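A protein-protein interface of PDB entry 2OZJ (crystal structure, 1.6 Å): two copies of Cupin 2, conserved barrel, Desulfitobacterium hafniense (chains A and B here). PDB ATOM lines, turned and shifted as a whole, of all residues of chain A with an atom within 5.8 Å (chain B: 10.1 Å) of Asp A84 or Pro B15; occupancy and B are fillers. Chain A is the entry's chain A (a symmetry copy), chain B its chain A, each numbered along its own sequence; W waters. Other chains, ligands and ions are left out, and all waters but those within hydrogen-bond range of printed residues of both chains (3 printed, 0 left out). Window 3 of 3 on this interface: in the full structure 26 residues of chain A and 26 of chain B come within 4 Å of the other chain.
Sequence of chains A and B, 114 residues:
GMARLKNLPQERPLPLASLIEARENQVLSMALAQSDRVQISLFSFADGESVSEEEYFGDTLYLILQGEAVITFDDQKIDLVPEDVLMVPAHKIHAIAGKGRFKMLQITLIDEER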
ATOM      1  N   TYR A  62      23.330  14.329  11.503  1.00  0.00           N
ATOM      2  CA  TYR A  62      22.729  15.680  11.501  1.00  0.00           C
ATOM      3  C   TYR A  62      23.129  16.394  12.811  1.00  0.00           C
ATOM      4  O   TYR A  62      23.020  15.831  13.911  1.00  0.00           O
ATOM      5  CB  TYR A  62      21.216  15.607  11.443  1.00  0.00           C
ATOM      6  CG  TYR A  62      20.688  15.046  10.179  1.00  0.00           C
ATOM      7  CD1 TYR A  62      20.737  15.788   9.029  1.00  0.00           C
ATOM      8  CD2 TYR A  62      20.136  13.778  10.119  1.00  0.00           C
ATOM      9  CE1 TYR A  62      20.254  15.289   7.840  1.00  0.00           C
ATOM     10  CE2 TYR A  62      19.646  13.265   8.908  1.00  0.00           C
ATOM     11  CZ  TYR A  62      19.712  14.033   7.789  1.00  0.00           C
ATOM     12  OH  TYR A  62      19.238  13.566   6.585  1.00  0.00           O
ATOM     13  N   LEU A  63      23.560  17.637  12.681  1.00  0.00           N
ATOM     14  CA  LEU A  63      23.907  18.497  13.811  1.00  0.00           C
ATOM     15  C   LEU A  63      23.159  19.806  13.674  1.00  0.00           C
ATOM     16  O   LEU A  63      23.325  20.514  12.675  1.00  0.00           O
ATOM     17  CB  LEU A  63      25.400  18.765  13.910  1.00  0.00           C
ATOM     18  CG  LEU A  63      25.870  19.770  14.977  1.00  0.00           C
ATOM     19  CD1 LEU A  63      25.777  19.285  16.455  1.00  0.00           C
ATOM     20  CD2 LEU A  63      27.358  20.097  14.648  1.00  0.00           C
ATOM     21  N   ILE A  64      22.298  20.103  14.656  1.00  0.00           N
ATOM     22  CA  ILE A  64      21.513  21.325  14.604  1.00  0.00           C
ATOM     23  C   ILE A  64      22.366  22.493  15.093  1.00  0.00           C
ATOM     24  O   ILE A  64      22.919  22.440  16.179  1.00  0.00           O
ATOM     25  CB  ILE A  64      20.220  21.232  15.417  1.00  0.00           C
ATOM     26  CG1 ILE A  64      19.452  19.982  15.037  1.00  0.00           C
ATOM     27  CG2 ILE A  64      19.337  22.486  15.172  1.00  0.00           C
ATOM     28  CD1 ILE A  64      19.105  19.893  13.598  1.00  0.00           C
ATOM     29  N   ASP A  79      12.251  15.323  18.066  1.00  0.00           N
ATOM     30  CA  ASP A  79      12.502  16.755  18.146  1.00  0.00           C
ATOM     31  C   ASP A  79      13.981  17.035  18.427  1.00  0.00           C
ATOM     32  O   ASP A  79      14.624  16.344  19.233  1.00  0.00           O
ATOM     33  CB  ASP A  79      11.662  17.394  19.265  1.00  0.00           C
ATOM     34  CG  ASP A  79      10.173  17.339  18.992  1.00  0.00           C
ATOM     35  OD1 ASP A  79       9.757  17.567  17.836  1.00  0.00           O
ATOM     36  OD2 ASP A  79       9.433  17.075  19.956  1.00  0.00           O
ATOM     37  N   LEU A  80      14.481  18.088  17.795  1.00  0.00           N
ATOM     38  CA  LEU A  80      15.869  18.503  17.934  1.00  0.00           C
ATOM     39  C   LEU A  80      15.976  19.993  18.245  1.00  0.00           C
ATOM     40  O   LEU A  80      15.161  20.818  17.771  1.00  0.00           O
ATOM     41  CB  LEU A  80      16.677  18.167  16.677  1.00  0.00           C
ATOM     42  CG  LEU A  80      16.847  16.673  16.329  1.00  0.00           C
ATOM     43  CD1 LEU A  80      15.853  16.309  15.224  1.00  0.00           C
ATOM     44  CD2 LEU A  80      18.270  16.314  15.895  1.00  0.00           C
ATOM     45  N   VAL A  81      16.964  20.333  19.069  1.00  0.00           N
ATOM     46  CA  VAL A  81      17.217  21.718  19.473  1.00  0.00           C
ATOM     47  C   VAL A  81      18.678  21.998  19.182  1.00  0.00           C
ATOM     48  O   VAL A  81      19.440  21.068  18.932  1.00  0.00           O
ATOM     49  CB  VAL A  81      16.856  21.942  20.967  1.00  0.00           C
ATOM     50  CG1 VAL A  81      15.405  21.566  21.216  1.00  0.00           C
ATOM     51  CG2 VAL A  81      17.796  21.173  21.888  1.00  0.00           C
ATOM     52  N   PRO A  82      19.086  23.271  19.194  1.00  0.00           N
ATOM     53  CA  PRO A  82      20.478  23.583  18.847  1.00  0.00           C
ATOM     54  C   PRO A  82      21.504  22.780  19.637  1.00  0.00           C
ATOM     55  O   PRO A  82      21.333  22.555  20.848  1.00  0.00           O
ATOM     56  CB  PRO A  82      20.579  25.081  19.153  1.00  0.00           C
ATOM     57  CG  PRO A  82      19.219  25.574  18.957  1.00  0.00           C
ATOM     58  CD  PRO A  82      18.323  24.494  19.507  1.00  0.00           C
ATOM     59  N   GLU A  83      22.553  22.361  18.937  1.00  0.00           N
ATOM     60  CA  GLU A  83      23.612  21.498  19.428  1.00  0.00           C
ATOM     61  C   GLU A  83      23.304  20.004  19.383  1.00  0.00           C
ATOM     62  O   GLU A  83      24.233  19.210  19.450  1.00  0.00           O
ATOM     63  CB  GLU A  83      24.137  21.875  20.828  1.00  0.00           C
ATOM     64  CG  GLU A  83      24.663  23.296  20.950  1.00  0.00           C
ATOM     65  CD  GLU A  83      25.128  23.608  22.364  1.00  0.00           C
ATOM     66  OE1 GLU A  83      25.472  22.659  23.106  1.00  0.00           O
ATOM     67  OE2 GLU A  83      25.148  24.796  22.746  1.00  0.00           O
ATOM     68  N   ASP A  84      22.046  19.597  19.257  1.00  0.00           N
ATOM     69  CA  ASP A  84      21.752  18.169  19.131  1.00  0.00           C
ATOM     70  C   ASP A  84      22.383  17.556  17.890  1.00  0.00           C
ATOM     71  O   ASP A  84      22.407  18.186  16.826  1.00  0.00           O
ATOM     72  CB  ASP A  84      20.244  17.919  19.054  1.00  0.00           C
ATOM     73  CG  ASP A  84      19.523  18.011  20.410  1.00  0.00           C
ATOM     74  OD1 ASP A  84      20.110  17.930  21.538  1.00  0.00           O
ATOM     75  OD2 ASP A  84      18.279  18.135  20.313  1.00  0.00           O
ATOM     76  N   VAL A  85      22.852  16.318  18.068  1.00  0.00           N
ATOM     77  CA  VAL A  85      23.298  15.447  17.019  1.00  0.00           C
ATOM     78  C   VAL A  85      22.423  14.202  17.028  1.00  0.00           C
ATOM     79  O   VAL A  85      21.961  13.706  18.099  1.00  0.00           O
ATOM     80  CB  VAL A  85      24.820  15.122  17.157  1.00  0.00           C
ATOM     81  CG1 VAL A  85      25.082  14.167  18.348  1.00  0.00           C
ATOM     82  CG2 VAL A  85      25.339  14.573  15.903  1.00  0.00           C
ATOM     83  N   LEU A  86      22.129  13.724  15.832  1.00  0.00           N
ATOM     84  CA  LEU A  86      21.460  12.442  15.643  1.00  0.00           C
ATOM     85  C   LEU A  86      22.057  11.757  14.433  1.00  0.00           C
ATOM     86  O   LEU A  86      22.272  12.406  13.411  1.00  0.00           O
ATOM     87  CB  LEU A  86      19.947  12.625  15.428  1.00  0.00           C
ATOM     88  CG  LEU A  86      19.094  11.357  15.632  1.00  0.00           C
ATOM     89  CD1 LEU A  86      19.030  10.853  17.090  1.00  0.00           C
ATOM     90  CD2 LEU A  86      17.677  11.602  15.146  1.00  0.00           C
ATOM     91  N   ASN B   7      29.110   5.444  17.469  1.00  0.00           N
ATOM     92  CA  ASN B   7      29.190   6.072  18.758  1.00  0.00           C
ATOM     93  C   ASN B   7      28.413   7.376  18.881  1.00  0.00           C
ATOM     94  O   ASN B   7      28.781   8.280  19.658  1.00  0.00           O
ATOM     95  CB  ASN B   7      30.655   6.247  19.193  1.00  0.00           C
ATOM     96  CG  ASN B   7      31.371   4.933  19.364  1.00  0.00           C
ATOM     97  OD1 ASN B   7      30.777   3.921  19.777  1.00  0.00           O
ATOM     98  ND2 ASN B   7      32.665   4.918  19.008  1.00  0.00           N
ATOM     99  N   LEU B   8      27.285   7.421  18.159  1.00  0.00           N
ATOM    100  CA  LEU B   8      26.407   8.590  18.111  1.00  0.00           C
ATOM    101  C   LEU B   8      24.978   8.181  18.374  1.00  0.00           C
ATOM    102  O   LEU B   8      24.582   7.058  17.980  1.00  0.00           O
ATOM    103  CB  LEU B   8      26.463   9.251  16.732  1.00  0.00           C
ATOM    104  CG  LEU B   8      27.773   9.962  16.382  1.00  0.00           C
ATOM    105  CD1 LEU B   8      27.927  10.055  14.850  1.00  0.00           C
ATOM    106  CD2 LEU B   8      27.805  11.323  17.081  1.00  0.00           C
ATOM    107  N   PRO B   9      24.200   9.066  19.030  1.00  0.00           N
ATOM    108  CA  PRO B   9      22.825   8.615  19.278  1.00  0.00           C
ATOM    109  C   PRO B   9      21.978   8.465  18.018  1.00  0.00           C
ATOM    110  O   PRO B   9      22.129   9.252  17.063  1.00  0.00           O
ATOM    111  CB  PRO B   9      22.250   9.705  20.173  1.00  0.00           C
ATOM    112  CG  PRO B   9      23.089  10.882  20.022  1.00  0.00           C
ATOM    113  CD  PRO B   9      24.436  10.442  19.516  1.00  0.00           C
ATOM    114  N   GLU B  11      18.470   7.279  18.551  1.00  0.00           N
ATOM    115  CA  GLU B  11      17.083   7.407  18.951  1.00  0.00           C
ATOM    116  C   GLU B  11      16.767   8.603  19.837  1.00  0.00           C
ATOM    117  O   GLU B  11      15.629   9.043  19.842  1.00  0.00           O
ATOM    118  CB  GLU B  11      16.607   6.141  19.664  1.00  0.00           C
ATOM    119  CG  GLU B  11      17.377   4.875  19.280  1.00  0.00           C
ATOM    120  CD  GLU B  11      16.560   3.630  19.414  1.00  0.00           C
ATOM    121  OE1 GLU B  11      15.333   3.671  19.109  1.00  0.00           O
ATOM    122  OE2 GLU B  11      17.138   2.594  19.846  1.00  0.00           O
ATOM    123  N   ARG B  12      17.719   9.063  20.649  1.00  0.00           N
ATOM    124  CA  ARG B  12      17.496  10.288  21.423  1.00  0.00           C
ATOM    125  C   ARG B  12      18.668  11.228  21.174  1.00  0.00           C
ATOM    126  O   ARG B  12      19.787  10.904  21.498  1.00  0.00           O
ATOM    127  CB  ARG B  12      17.231   9.991  22.919  1.00  0.00           C
ATOM    128  CG  ARG B  12      18.028  10.809  23.983  1.00  0.00           C
ATOM    129  CD  ARG B  12      17.776  10.238  25.392  1.00  0.00           C
ATOM    130  NE  ARG B  12      16.335  10.244  25.711  1.00  0.00           N
ATOM    131  CZ  ARG B  12      15.819   9.696  26.798  1.00  0.00           C
ATOM    132  NH1 ARG B  12      16.691   9.166  27.615  1.00  0.00           N
ATOM    133  NH2 ARG B  12      14.493   9.748  27.024  1.00  0.00           N
ATOM    134  N   PRO B  13      18.396  12.388  20.577  1.00  0.00           N
ATOM    135  CA  PRO B  13      19.451  13.339  20.269  1.00  0.00           C
ATOM    136  C   PRO B  13      20.105  13.867  21.547  1.00  0.00           C
ATOM    137  O   PRO B  13      19.436  13.974  22.606  1.00  0.00           O
ATOM    138  CB  PRO B  13      18.697  14.455  19.538  1.00  0.00           C
ATOM    139  CG  PRO B  13      17.336  14.403  20.087  1.00  0.00           C
ATOM    140  CD  PRO B  13      17.063  12.938  20.268  1.00  0.00           C
ATOM    141  N   LEU B  14      21.389  14.152  21.448  1.00  0.00           N
ATOM    142  CA  LEU B  14      22.150  14.688  22.550  1.00  0.00           C
ATOM    143  C   LEU B  14      23.062  15.742  21.963  1.00  0.00           C
ATOM    144  O   LEU B  14      23.469  15.621  20.817  1.00  0.00           O
ATOM    145  CB  LEU B  14      22.986  13.598  23.239  1.00  0.00           C
ATOM    146  CG  LEU B  14      22.261  12.379  23.830  1.00  0.00           C
ATOM    147  CD1 LEU B  14      23.276  11.287  24.208  1.00  0.00           C
ATOM    148  CD2 LEU B  14      21.424  12.768  25.016  1.00  0.00           C
ATOM    149  N   PRO B  15      23.444  16.723  22.785  1.00  0.00           N
ATOM    150  CA  PRO B  15      24.459  17.659  22.378  1.00  0.00           C
ATOM    151  C   PRO B  15      25.771  16.926  22.227  1.00  0.00           C
ATOM    152  O   PRO B  15      26.134  16.056  23.038  1.00  0.00           O
ATOM    153  CB  PRO B  15      24.545  18.626  23.567  1.00  0.00           C
ATOM    154  CG  PRO B  15      23.496  18.282  24.465  1.00  0.00           C
ATOM    155  CD  PRO B  15      22.986  16.952  24.156  1.00  0.00           C
ATOM    156  N   LEU B  16      26.520  17.306  21.216  1.00  0.00           N
ATOM    157  CA  LEU B  16      27.719  16.650  20.885  1.00  0.00           C
ATOM    158  C   LEU B  16      28.759  16.741  22.029  1.00  0.00           C
ATOM    159  O   LEU B  16      29.415  15.759  22.403  1.00  0.00           O
ATOM    160  CB  LEU B  16      28.206  17.287  19.578  1.00  0.00           C
ATOM    161  CG  LEU B  16      29.203  16.556  18.752  1.00  0.00           C
ATOM    162  CD1 LEU B  16      28.828  15.127  18.400  1.00  0.00           C
ATOM    163  CD2 LEU B  16      29.378  17.465  17.471  1.00  0.00           C
ATOM    164  N   ALA B  17      28.792  17.901  22.694  1.00  0.00           N
ATOM    165  CA  ALA B  17      29.686  18.108  23.836  1.00  0.00           C
ATOM    166  C   ALA B  17      29.398  17.132  24.975  1.00  0.00           C
ATOM    167  O   ALA B  17      30.275  16.791  25.764  1.00  0.00           O
ATOM    168  CB  ALA B  17      29.552  19.527  24.357  1.00  0.00           C
ATOM    169  N   SER B  18      28.153  16.691  25.097  1.00  0.00           N
ATOM    170  CA  SER B  18      27.774  15.797  26.186  1.00  0.00           C
ATOM    171  C   SER B  18      28.294  14.355  25.987  1.00  0.00           C
ATOM    172  O   SER B  18      28.196  13.553  26.909  1.00  0.00           O
ATOM    173  CB  SER B  18      26.246  15.838  26.423  1.00  0.00           C
ATOM    174  OG  SER B  18      25.590  15.066  25.466  1.00  0.00           O
ATOM    175  N   LEU B  19      28.824  14.017  24.813  1.00  0.00           N
ATOM    176  CA  LEU B  19      29.245  12.660  24.510  1.00  0.00           C
ATOM    177  C   LEU B  19      30.682  12.370  25.012  1.00  0.00           C
ATOM    178  O   LEU B  19      31.092  11.231  25.015  1.00  0.00           O
ATOM    179  CB  LEU B  19      29.153  12.357  23.029  1.00  0.00           C
ATOM    180  CG  LEU B  19      27.752  12.448  22.392  1.00  0.00           C
ATOM    181  CD1 LEU B  19      27.921  12.152  20.918  1.00  0.00           C
ATOM    182  CD2 LEU B  19      26.759  11.514  23.038  1.00  0.00           C
ATOM    183  N   ILE B  20      31.396  13.400  25.457  1.00  0.00           N
ATOM    184  CA  ILE B  20      32.767  13.242  25.971  1.00  0.00           C
ATOM    185  C   ILE B  20      32.967  14.135  27.205  1.00  0.00           C
ATOM    186  O   ILE B  20      32.530  15.285  27.227  1.00  0.00           O
ATOM    187  CB  ILE B  20      33.831  13.503  24.861  1.00  0.00           C
ATOM    188  CG1 ILE B  20      35.205  12.940  25.233  1.00  0.00           C
ATOM    189  CG2 ILE B  20      33.975  14.985  24.493  1.00  0.00           C
ATOM    190  CD1 ILE B  20      36.133  12.861  24.031  1.00  0.00           C
ATOM    191  N   GLU B  21      33.619  13.614  28.233  1.00  0.00           N
ATOM    192  CA  GLU B  21      34.004  14.453  29.370  1.00  0.00           C
ATOM    193  C   GLU B  21      35.253  15.271  29.066  1.00  0.00           C
ATOM    194  O   GLU B  21      35.920  15.027  28.073  1.00  0.00           O
ATOM    195  CB  GLU B  21      34.228  13.596  30.611  1.00  0.00           C
ATOM    196  CG  GLU B  21      32.943  12.891  31.018  1.00  0.00           C
ATOM    197  CD  GLU B  21      33.191  11.623  31.826  1.00  0.00           C
ATOM    198  OE1 GLU B  21      33.712  10.633  31.268  1.00  0.00           O
ATOM    199  OE2 GLU B  21      32.861  11.622  33.014  1.00  0.00           O
ATOM    200  N   MET B  30      37.206   9.805  21.171  1.00  0.00           N
ATOM    201  CA  MET B  30      36.186   8.869  20.719  1.00  0.00           C
ATOM    202  C   MET B  30      36.060   8.957  19.210  1.00  0.00           C
ATOM    203  O   MET B  30      35.905  10.082  18.693  1.00  0.00           O
ATOM    204  CB  MET B  30      34.853   9.173  21.395  1.00  0.00           C
ATOM    205  CG  MET B  30      33.799   8.128  21.039  1.00  0.00           C
ATOM    206  SD  MET B  30      32.285   7.984  22.200  1.00  0.00           S
ATOM    207  CE  MET B  30      31.421   9.638  21.663  1.00  0.00           C
ATOM    208  N   LEU B  32      34.065   8.616  15.805  1.00  0.00           N
ATOM    209  CA  LEU B  32      32.676   8.671  15.347  1.00  0.00           C
ATOM    210  C   LEU B  32      32.499   8.072  13.963  1.00  0.00           C
ATOM    211  O   LEU B  32      31.401   8.056  13.442  1.00  0.00           O
ATOM    212  CB  LEU B  32      32.167  10.104  15.347  1.00  0.00           C
ATOM    213  CG  LEU B  32      32.283  10.942  16.646  1.00  0.00           C
ATOM    214  CD1 LEU B  32      31.699  12.351  16.417  1.00  0.00           C
ATOM    215  CD2 LEU B  32      31.641  10.211  17.858  1.00  0.00           C
ATOM    216  N   LEU B  42      35.985  12.877  18.349  1.00  0.00           N
ATOM    217  CA  LEU B  42      35.821  13.831  19.447  1.00  0.00           C
ATOM    218  C   LEU B  42      37.063  13.738  20.346  1.00  0.00           C
ATOM    219  O   LEU B  42      37.533  12.635  20.633  1.00  0.00           O
ATOM    220  CB  LEU B  42      34.592  13.526  20.310  1.00  0.00           C
ATOM    221  CG  LEU B  42      33.212  13.746  19.753  1.00  0.00           C
ATOM    222  CD1 LEU B  42      32.170  13.496  20.866  1.00  0.00           C
ATOM    223  CD2 LEU B  42      33.130  15.164  19.079  1.00  0.00           C
ATOM    224  N   LEU B  63      36.209  21.910  15.037  1.00  0.00           N
ATOM    225  CA  LEU B  63      35.031  22.586  15.579  1.00  0.00           C
ATOM    226  C   LEU B  63      35.097  22.540  17.091  1.00  0.00           C
ATOM    227  O   LEU B  63      35.137  21.452  17.677  1.00  0.00           O
ATOM    228  CB  LEU B  63      33.727  21.970  15.101  1.00  0.00           C
ATOM    229  CG  LEU B  63      32.422  22.509  15.715  1.00  0.00           C
ATOM    230  CD1 LEU B  63      32.002  23.941  15.269  1.00  0.00           C
ATOM    231  CD2 LEU B  63      31.299  21.507  15.310  1.00  0.00           C
ATOM    232  N   LEU B  65      33.697  22.634  20.647  1.00  0.00           N
ATOM    233  CA  LEU B  65      32.405  22.326  21.227  1.00  0.00           C
ATOM    234  C   LEU B  65      32.210  23.032  22.571  1.00  0.00           C
ATOM    235  O   LEU B  65      31.103  23.439  22.923  1.00  0.00           O
ATOM    236  CB  LEU B  65      32.260  20.820  21.421  1.00  0.00           C
ATOM    237  CG  LEU B  65      32.409  19.980  20.155  1.00  0.00           C
ATOM    238  CD1 LEU B  65      32.348  18.509  20.519  1.00  0.00           C
ATOM    239  CD2 LEU B  65      31.368  20.349  19.091  1.00  0.00           C
ATOM    240  N   GLN B  66      33.290  23.176  23.328  1.00  0.00           N
ATOM    241  CA  GLN B  66      33.229  23.681  24.678  1.00  0.00           C
ATOM    242  C   GLN B  66      34.641  24.097  25.035  1.00  0.00           C
ATOM    243  O   GLN B  66      35.600  23.483  24.602  1.00  0.00           O
ATOM    244  CB  GLN B  66      32.749  22.549  25.572  1.00  0.00           C
ATOM    245  CG  GLN B  66      32.313  22.907  26.958  1.00  0.00           C
ATOM    246  CD  GLN B  66      32.011  21.648  27.776  1.00  0.00           C
ATOM    247  OE1 GLN B  66      31.064  20.906  27.486  1.00  0.00           O
ATOM    248  NE2 GLN B  66      32.834  21.396  28.798  1.00  0.00           N
ATOM    249  N   LYS B 103      36.757  20.789  24.496  1.00  0.00           N
ATOM    250  CA  LYS B 103      36.291  19.679  23.749  1.00  0.00           C
ATOM    251  C   LYS B 103      36.187  20.101  22.293  1.00  0.00           C
ATOM    252  O   LYS B 103      35.763  21.227  21.991  1.00  0.00           O
ATOM    253  CB  LYS B 103      34.910  19.267  24.220  1.00  0.00           C
ATOM    254  CG  LYS B 103      34.820  18.811  25.659  1.00  0.00           C
ATOM    255  CD  LYS B 103      33.363  18.544  26.029  1.00  0.00           C
ATOM    256  CE  LYS B 103      33.201  18.230  27.520  1.00  0.00           C
ATOM    257  NZ  LYS B 103      31.767  18.010  27.880  1.00  0.00           N
HETATM  258  O   HOH W   1      26.873  19.776  19.421  1.00  0.00           O
HETATM  259  O   HOH W   2      19.167  17.236  23.703  1.00  0.00           O
HETATM  260  O   HOH W   3      27.677  20.384  21.730  1.00  0.00           O
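O of Leu B14 is in hydrogen-bond range of N of Val A85, 2.9 Å away. The backbone NH (N) of Leu B16 is in hydrogen-bond range of the backbone carbonyl oxygen (O) of Glu A83 (3.5 Å).
The backbone carbonyl oxygen (O) of Pro B15 sits at hydrogen-bond distance from the side-chain hydroxyl (OG) of Ser B18. The backbone NH of Tyr A62 is in hydrogen-bond range of the backbone carbonyl oxygen of Leu A86, at 2.9 Å. The backbone carbonyl oxygen (O) of Ile A64 sits at hydrogen-bond distance from the backbone NH (N) of Glu A83, 2.8 Å away. The backbone NH (N) of Ile A64 sits at hydrogen-bond distance from the backbone carbonyl oxygen (O) of Asp A84. The backbone NH (N) of Val A81 lies within hydrogen-bond range of the side-chain carboxylate (OD2) of Asp A84, 2.8 Å away.
Among the printed residues, pairs that only touch across the chains: Glu A83 with Pro B15, Val A85 with Pro B13, Asp A79 with Pro B13, Leu A86 with Pro B9, Asp A84 with Leu B14, Val A85 with Pro B9, Asp A84 with Pro B13, Asp A84 with Pro B15, Leu A86 with Pro B13, Val A85 with Leu B16, Leu A86 with Glu B11 and Glu A83 with Leu B14.
No residue of chain B comes within 4 Å of Leu A63. No residue of chain B comes within 4 Å of Ile A64. Printed residues of chain B within 4 Å of Asp A79: Pro B13. No residue of chain B comes within 4 Å of Val A81. Printed residues of chain B within 4 Å of Val A85: Pro B9 (3.6 Å), Pro B13 (3.3 Å), Leu B14 (2.9 Å) and Leu B16 (3.9 Å). Of the printed residues of chain A, Glu B11 touches Leu A86. Printed residues of chain A within 4 Å of Pro B13: Asp A79, Asp A84, Val A85 and Leu A86. Of the printed residues of chain A, Leu B14 touches Glu A83 (3.9 Å), Asp A84 (3.5 Å) and Val A85 (2.9 Å). Pro B15 touches just these residues of chain A: Glu A83 (3.3 Å) and Asp A84 (3.8 Å). The nearest printed residue of chain B that does not touch Leu A86 is Arg B12 (4.1 Å).
Of the 21 printed residues of chain B, 6 touch a printed residue of chain A. Hydrophobic or aromatic side chains of chain A within 4 Å of the printed part of chain B: Val A85 and Leu A86.
1 position is printed for both chains. Of the 14 pairs that touch across the chains among the printed residues, none has its exchanged pair printed and touching as well.
Water W2 bridges the side-chain carboxylate (OD1) of Asp A84 (2.5 Å) and the backbone carbonyl oxygen (O) of Pro B13 (3.5 Å). Water W1 bridges the backbone carbonyl oxygen (O) of Glu A83 (2.7 Å) and the backbone NH (N) of Leu B16 (3.1 Å). Water W3 lies within hydrogen-bond range of N of Ala B17, N of Leu B16 and OE1 of Glu A83.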
